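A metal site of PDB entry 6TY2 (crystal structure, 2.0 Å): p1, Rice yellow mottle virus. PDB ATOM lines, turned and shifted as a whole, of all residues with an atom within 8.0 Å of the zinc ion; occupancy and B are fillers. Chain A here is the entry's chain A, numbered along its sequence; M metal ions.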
ATOM      1  N   GLU A   3      10.107  18.545 -12.044  1.00  0.00           N
ATOM      2  CA  GLU A   3      10.331  19.493 -13.130  1.00  0.00           C
ATOM      3  C   GLU A   3      11.505  19.049 -13.999  1.00  0.00           C
ATOM      4  O   GLU A   3      11.486  19.267 -15.213  1.00  0.00           O
ATOM      5  CB  GLU A   3      10.570  20.887 -12.574  1.00  0.00           C
ATOM      6  CG  GLU A   3      10.793  21.945 -13.636  1.00  0.00           C
ATOM      7  CD  GLU A   3       9.658  22.047 -14.661  1.00  0.00           C
ATOM      8  OE1 GLU A   3       8.473  21.808 -14.294  1.00  0.00           O
ATOM      9  OE2 GLU A   3       9.958  22.395 -15.826  1.00  0.00           O
ATOM     10  N   ILE A   4      12.506  18.418 -13.395  1.00  0.00           N
ATOM     11  CA  ILE A   4      13.581  17.728 -14.127  1.00  0.00           C
ATOM     12  C   ILE A   4      13.037  16.784 -15.184  1.00  0.00           C
ATOM     13  O   ILE A   4      13.489  16.792 -16.327  1.00  0.00           O
ATOM     14  CB  ILE A   4      14.460  16.895 -13.159  1.00  0.00           C
ATOM     15  CG1 ILE A   4      15.196  17.806 -12.180  1.00  0.00           C
ATOM     16  CG2 ILE A   4      15.449  16.028 -13.929  1.00  0.00           C
ATOM     17  CD1 ILE A   4      16.568  18.213 -12.625  1.00  0.00           C
ATOM     18  N   ASP A   5      12.067  15.970 -14.787  1.00  0.00           N
ATOM     19  CA  ASP A   5      11.481  14.995 -15.697  1.00  0.00           C
ATOM     20  C   ASP A   5      10.741  15.664 -16.831  1.00  0.00           C
ATOM     21  O   ASP A   5      10.782  15.219 -17.974  1.00  0.00           O
ATOM     22  CB  ASP A   5      10.540  14.074 -14.932  1.00  0.00           C
ATOM     23  CG  ASP A   5      11.220  13.373 -13.797  1.00  0.00           C
ATOM     24  OD1 ASP A   5      11.927  12.381 -14.061  1.00  0.00           O
ATOM     25  OD2 ASP A   5      11.058  13.814 -12.628  1.00  0.00           O
ATOM     26  N   GLU A   7      11.354  18.533 -18.195  1.00  0.00           N
ATOM     27  CA  GLU A   7      12.281  19.075 -19.188  1.00  0.00           C
ATOM     28  C   GLU A   7      12.945  17.977 -20.023  1.00  0.00           C
ATOM     29  O   GLU A   7      13.275  18.197 -21.184  1.00  0.00           O
ATOM     30  CB  GLU A   7      13.348  19.941 -18.508  1.00  0.00           C
ATOM     31  CG  GLU A   7      12.807  21.308 -18.092  1.00  0.00           C
ATOM     32  CD  GLU A   7      13.805  22.137 -17.302  1.00  0.00           C
ATOM     33  OE1 GLU A   7      13.795  23.379 -17.418  1.00  0.00           O
ATOM     34  OE2 GLU A   7      14.609  21.550 -16.553  1.00  0.00           O
ATOM     35  N   HIS A   8      13.130  16.791 -19.447  1.00  0.00           N
ATOM     36  CA  HIS A   8      13.614  15.650 -20.232  1.00  0.00           C
ATOM     37  C   HIS A   8      12.577  15.265 -21.289  1.00  0.00           C
ATOM     38  O   HIS A   8      12.934  14.961 -22.430  1.00  0.00           O
ATOM     39  CB  HIS A   8      13.915  14.453 -19.343  1.00  0.00           C
ATOM     40  CG  HIS A   8      15.109  14.634 -18.476  1.00  0.00           C
ATOM     41  ND1 HIS A   8      15.372  13.798 -17.409  1.00  0.00           N
ATOM     42  CD2 HIS A   8      16.121  15.537 -18.508  1.00  0.00           C
ATOM     43  CE1 HIS A   8      16.493  14.183 -16.819  1.00  0.00           C
ATOM     44  NE2 HIS A   8      16.972  15.232 -17.469  1.00  0.00           N
ATOM     45  N   LEU A  34      17.459  11.765 -23.525  1.00  0.00           N
ATOM     46  CA  LEU A  34      17.954  12.097 -22.195  1.00  0.00           C
ATOM     47  C   LEU A  34      17.286  11.280 -21.075  1.00  0.00           C
ATOM     48  O   LEU A  34      16.105  10.922 -21.152  1.00  0.00           O
ATOM     49  CB  LEU A  34      17.723  13.581 -21.905  1.00  0.00           C
ATOM     50  CG  LEU A  34      18.585  14.671 -22.528  1.00  0.00           C
ATOM     51  CD1 LEU A  34      18.544  14.646 -24.041  1.00  0.00           C
ATOM     52  CD2 LEU A  34      18.068  16.009 -22.020  1.00  0.00           C
ATOM     53  N   SER A  35      18.056  11.003 -20.023  1.00  0.00           N
ATOM     54  CA  SER A  35      17.504  10.521 -18.758  1.00  0.00           C
ATOM     55  C   SER A  35      18.323  11.149 -17.658  1.00  0.00           C
ATOM     56  O   SER A  35      19.313  11.820 -17.932  1.00  0.00           O
ATOM     57  CB  SER A  35      17.550   8.998 -18.659  1.00  0.00           C
ATOM     58  OG  SER A  35      18.890   8.547 -18.619  1.00  0.00           O
ATOM     59  N   ARG A  36      17.935  10.915 -16.403  1.00  0.00           N
ATOM     60  CA  ARG A  36      18.707  11.393 -15.273  1.00  0.00           C
ATOM     61  C   ARG A  36      20.114  10.846 -15.300  1.00  0.00           C
ATOM     62  O   ARG A  36      21.037  11.462 -14.781  1.00  0.00           O
ATOM     63  CB  ARG A  36      18.032  11.029 -13.948  1.00  0.00           C
ATOM     64  CG  ARG A  36      16.700  11.735 -13.719  1.00  0.00           C
ATOM     65  CD  ARG A  36      16.099  11.390 -12.365  1.00  0.00           C
ATOM     66  NE  ARG A  36      14.735  11.906 -12.235  1.00  0.00           N
ATOM     67  CZ  ARG A  36      14.018  11.857 -11.111  1.00  0.00           C
ATOM     68  NH1 ARG A  36      14.538  11.318 -10.016  1.00  0.00           N
ATOM     69  NH2 ARG A  36      12.792  12.359 -11.088  1.00  0.00           N
ATOM     70  N   ASP A  37      20.305   9.687 -15.916  1.00  0.00           N
ATOM     71  CA  ASP A  37      21.615   9.051 -15.894  1.00  0.00           C
ATOM     72  C   ASP A  37      22.513   9.409 -17.086  1.00  0.00           C
ATOM     73  O   ASP A  37      23.661   8.956 -17.163  1.00  0.00           O
ATOM     74  CB  ASP A  37      21.439   7.540 -15.779  1.00  0.00           C
ATOM     75  CG  ASP A  37      20.638   7.159 -14.545  1.00  0.00           C
ATOM     76  OD1 ASP A  37      20.996   7.601 -13.413  1.00  0.00           O
ATOM     77  OD2 ASP A  37      19.643   6.431 -14.707  1.00  0.00           O
ATOM     78  N   ALA A  38      22.003  10.229 -18.003  1.00  0.00           N
ATOM     79  CA  ALA A  38      22.825  10.832 -19.052  1.00  0.00           C
ATOM     80  C   ALA A  38      22.042  11.979 -19.646  1.00  0.00           C
ATOM     81  O   ALA A  38      21.109  11.777 -20.417  1.00  0.00           O
ATOM     82  CB  ALA A  38      23.208   9.809 -20.130  1.00  0.00           C
ATOM     83  N   CYS A  39      22.433  13.200 -19.272  1.00  0.00           N
ATOM     84  CA  CYS A  39      21.665  14.407 -19.562  1.00  0.00           C
ATOM     85  C   CYS A  39      22.573  15.552 -20.024  1.00  0.00           C
ATOM     86  O   CYS A  39      23.656  15.732 -19.490  1.00  0.00           O
ATOM     87  CB  CYS A  39      20.887  14.777 -18.307  1.00  0.00           C
ATOM     88  SG  CYS A  39      20.122  16.362 -18.284  1.00  0.00           S
ATOM     89  N   ASP A  40      22.135  16.343 -21.003  1.00  0.00           N
ATOM     90  CA  ASP A  40      23.029  17.391 -21.496  1.00  0.00           C
ATOM     91  C   ASP A  40      22.492  18.792 -21.203  1.00  0.00           C
ATOM     92  O   ASP A  40      22.872  19.753 -21.850  1.00  0.00           O
ATOM     93  CB  ASP A  40      23.303  17.221 -22.999  1.00  0.00           C
ATOM     94  CG  ASP A  40      22.045  17.278 -23.852  1.00  0.00           C
ATOM     95  OD1 ASP A  40      20.949  17.436 -23.296  1.00  0.00           O
ATOM     96  OD2 ASP A  40      22.153  17.147 -25.104  1.00  0.00           O
ATOM     97  N   ILE A  41      21.628  18.895 -20.203  1.00  0.00           N
ATOM     98  CA  ILE A  41      21.125  20.194 -19.756  1.00  0.00           C
ATOM     99  C   ILE A  41      21.964  20.683 -18.578  1.00  0.00           C
ATOM    100  O   ILE A  41      21.864  20.143 -17.489  1.00  0.00           O
ATOM    101  CB  ILE A  41      19.655  20.111 -19.349  1.00  0.00           C
ATOM    102  CG1 ILE A  41      18.836  19.428 -20.450  1.00  0.00           C
ATOM    103  CG2 ILE A  41      19.105  21.492 -19.017  1.00  0.00           C
ATOM    104  CD1 ILE A  41      17.385  19.219 -20.067  1.00  0.00           C
ATOM    105  N   PRO A  42      22.818  21.689 -18.808  1.00  0.00           N
ATOM    106  CA  PRO A  42      23.774  22.118 -17.773  1.00  0.00           C
ATOM    107  C   PRO A  42      23.116  22.467 -16.453  1.00  0.00           C
ATOM    108  O   PRO A  42      23.672  22.180 -15.404  1.00  0.00           O
ATOM    109  CB  PRO A  42      24.433  23.353 -18.391  1.00  0.00           C
ATOM    110  CG  PRO A  42      24.280  23.146 -19.865  1.00  0.00           C
ATOM    111  CD  PRO A  42      22.938  22.491 -20.032  1.00  0.00           C
ATOM    112  N   GLU A  43      21.930  23.061 -16.533  1.00  0.00           N
ATOM    113  CA  GLU A  43      21.190  23.486 -15.348  1.00  0.00           C
ATOM    114  C   GLU A  43      20.863  22.296 -14.458  1.00  0.00           C
ATOM    115  O   GLU A  43      20.729  22.422 -13.243  1.00  0.00           O
ATOM    116  CB  GLU A  43      19.905  24.222 -15.764  1.00  0.00           C
ATOM    117  CG  GLU A  43      20.125  25.565 -16.494  1.00  0.00           C
ATOM    118  CD  GLU A  43      20.562  25.406 -17.944  1.00  0.00           C
ATOM    119  OE1 GLU A  43      20.464  24.297 -18.498  1.00  0.00           O
ATOM    120  OE2 GLU A  43      21.027  26.395 -18.544  1.00  0.00           O
ATOM    121  N   HIS A  44      20.739  21.116 -15.062  1.00  0.00           N
ATOM    122  CA  HIS A  44      20.449  19.891 -14.323  1.00  0.00           C
ATOM    123  C   HIS A  44      21.669  19.279 -13.622  1.00  0.00           C
ATOM    124  O   HIS A  44      21.524  18.334 -12.858  1.00  0.00           O
ATOM    125  CB  HIS A  44      19.853  18.836 -15.239  1.00  0.00           C
ATOM    126  CG  HIS A  44      18.446  19.119 -15.670  1.00  0.00           C
ATOM    127  ND1 HIS A  44      17.703  18.209 -16.390  1.00  0.00           N
ATOM    128  CD2 HIS A  44      17.642  20.186 -15.468  1.00  0.00           C
ATOM    129  CE1 HIS A  44      16.503  18.708 -16.615  1.00  0.00           C
ATOM    130  NE2 HIS A  44      16.440  19.910 -16.067  1.00  0.00           N
ATOM    131  N   SER A  45      22.862  19.791 -13.913  1.00  0.00           N
ATOM    132  CA  SER A  45      24.092  19.144 -13.491  1.00  0.00           C
ATOM    133  C   SER A  45      24.105  18.898 -11.996  1.00  0.00           C
ATOM    134  O   SER A  45      23.777  19.780 -11.220  1.00  0.00           O
ATOM    135  CB  SER A  45      25.305  19.998 -13.893  1.00  0.00           C
ATOM    136  OG  SER A  45      26.472  19.201 -13.951  1.00  0.00           O
ATOM    137  N   GLY A  46      24.466  17.686 -11.609  1.00  0.00           N
ATOM    138  CA  GLY A  46      24.431  17.265 -10.222  1.00  0.00           C
ATOM    139  C   GLY A  46      23.250  16.367  -9.951  1.00  0.00           C
ATOM    140  O   GLY A  46      23.397  15.202  -9.544  1.00  0.00           O
ATOM    141  N   ARG A  47      22.056  16.892 -10.161  1.00  0.00           N
ATOM    142  CA  ARG A  47      20.875  16.090 -10.015  1.00  0.00           C
ATOM    143  C   ARG A  47      20.836  15.099 -11.174  1.00  0.00           C
ATOM    144  O   ARG A  47      20.466  13.954 -10.978  1.00  0.00           O
ATOM    145  CB  ARG A  47      19.638  16.978  -9.971  1.00  0.00           C
ATOM    146  CG  ARG A  47      19.613  17.891  -8.768  1.00  0.00           C
ATOM    147  CD  ARG A  47      18.445  18.869  -8.834  1.00  0.00           C
ATOM    148  NE  ARG A  47      18.652  19.835  -9.905  1.00  0.00           N
ATOM    149  CZ  ARG A  47      17.787  20.777 -10.228  1.00  0.00           C
ATOM    150  NH1 ARG A  47      16.650  20.875  -9.570  1.00  0.00           N
ATOM    151  NH2 ARG A  47      18.065  21.621 -11.217  1.00  0.00           N
ATOM    152  N   CYS A  48      21.255  15.529 -12.353  1.00  0.00           N
ATOM    153  CA  CYS A  48      21.453  14.604 -13.484  1.00  0.00           C
ATOM    154  C   CYS A  48      22.942  14.374 -13.760  1.00  0.00           C
ATOM    155  O   CYS A  48      23.786  15.192 -13.395  1.00  0.00           O
ATOM    156  CB  CYS A  48      20.773  15.132 -14.747  1.00  0.00           C
ATOM    157  SG  CYS A  48      18.990  15.162 -14.599  1.00  0.00           S
ATOM    158  N   ARG A  49      23.272  13.250 -14.390  1.00  0.00           N
ATOM    159  CA  ARG A  49      24.640  13.043 -14.844  1.00  0.00           C
ATOM    160  C   ARG A  49      24.867  13.890 -16.077  1.00  0.00           C
ATOM    161  O   ARG A  49      24.286  13.622 -17.123  1.00  0.00           O
ATOM    162  CB  ARG A  49      24.919  11.582 -15.153  1.00  0.00           C
ATOM    163  CG  ARG A  49      26.364  11.314 -15.498  1.00  0.00           C
ATOM    164  CD  ARG A  49      26.626   9.831 -15.600  1.00  0.00           C
ATOM    165  NE  ARG A  49      28.030   9.543 -15.854  1.00  0.00           N
ATOM    166  CZ  ARG A  49      28.551   8.317 -15.857  1.00  0.00           C
ATOM    167  NH1 ARG A  49      27.780   7.264 -15.628  1.00  0.00           N
ATOM    168  NH2 ARG A  49      29.841   8.154 -16.092  1.00  0.00           N
ATOM    169  N   PHE A  50      25.720  14.892 -15.967  1.00  0.00           N
ATOM    170  CA  PHE A  50      25.906  15.825 -17.061  1.00  0.00           C
ATOM    171  C   PHE A  50      26.881  15.265 -18.075  1.00  0.00           C
ATOM    172  O   PHE A  50      28.051  15.012 -17.795  1.00  0.00           O
ATOM    173  CB  PHE A  50      26.382  17.180 -16.526  1.00  0.00           C
ATOM    174  CG  PHE A  50      26.506  18.250 -17.573  1.00  0.00           C
ATOM    175  CD1 PHE A  50      25.486  18.479 -18.466  1.00  0.00           C
ATOM    176  CD2 PHE A  50      27.634  19.038 -17.635  1.00  0.00           C
ATOM    177  CE1 PHE A  50      25.588  19.461 -19.424  1.00  0.00           C
ATOM    178  CE2 PHE A  50      27.752  20.026 -18.584  1.00  0.00           C
ATOM    179  CZ  PHE A  50      26.732  20.243 -19.488  1.00  0.00           C
HETATM  180 ZN    ZN M   1      18.566  16.195 -16.604  1.00  0.00          ZN
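A ring nitrogen (NE2) of His 44 lies within hydrogen-bond range of the side-chain carboxylate (OE2) of Glu 7 (2.5 Å). The backbone NH of Cys 39 lies within hydrogen-bond range of the backbone carbonyl oxygen of Arg 49 (2.9 Å). The backbone NH (N) of Ile 41 lies close to the side-chain sulfur (SG) of Cys 39, 3.5 Å away.
Within 4 Å of the zinc ion: His 8, Cys 39, His 44 and Cys 48.
A ring nitrogen (NE2) of His 8 is bound to the zinc ion. ND1 of His 44 is bound to the zinc ion, 2.2 Å away. The zinc ion is bound by SG of Cys 48. SG of Cys 39 binds the zinc ion, at 2.3 Å.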
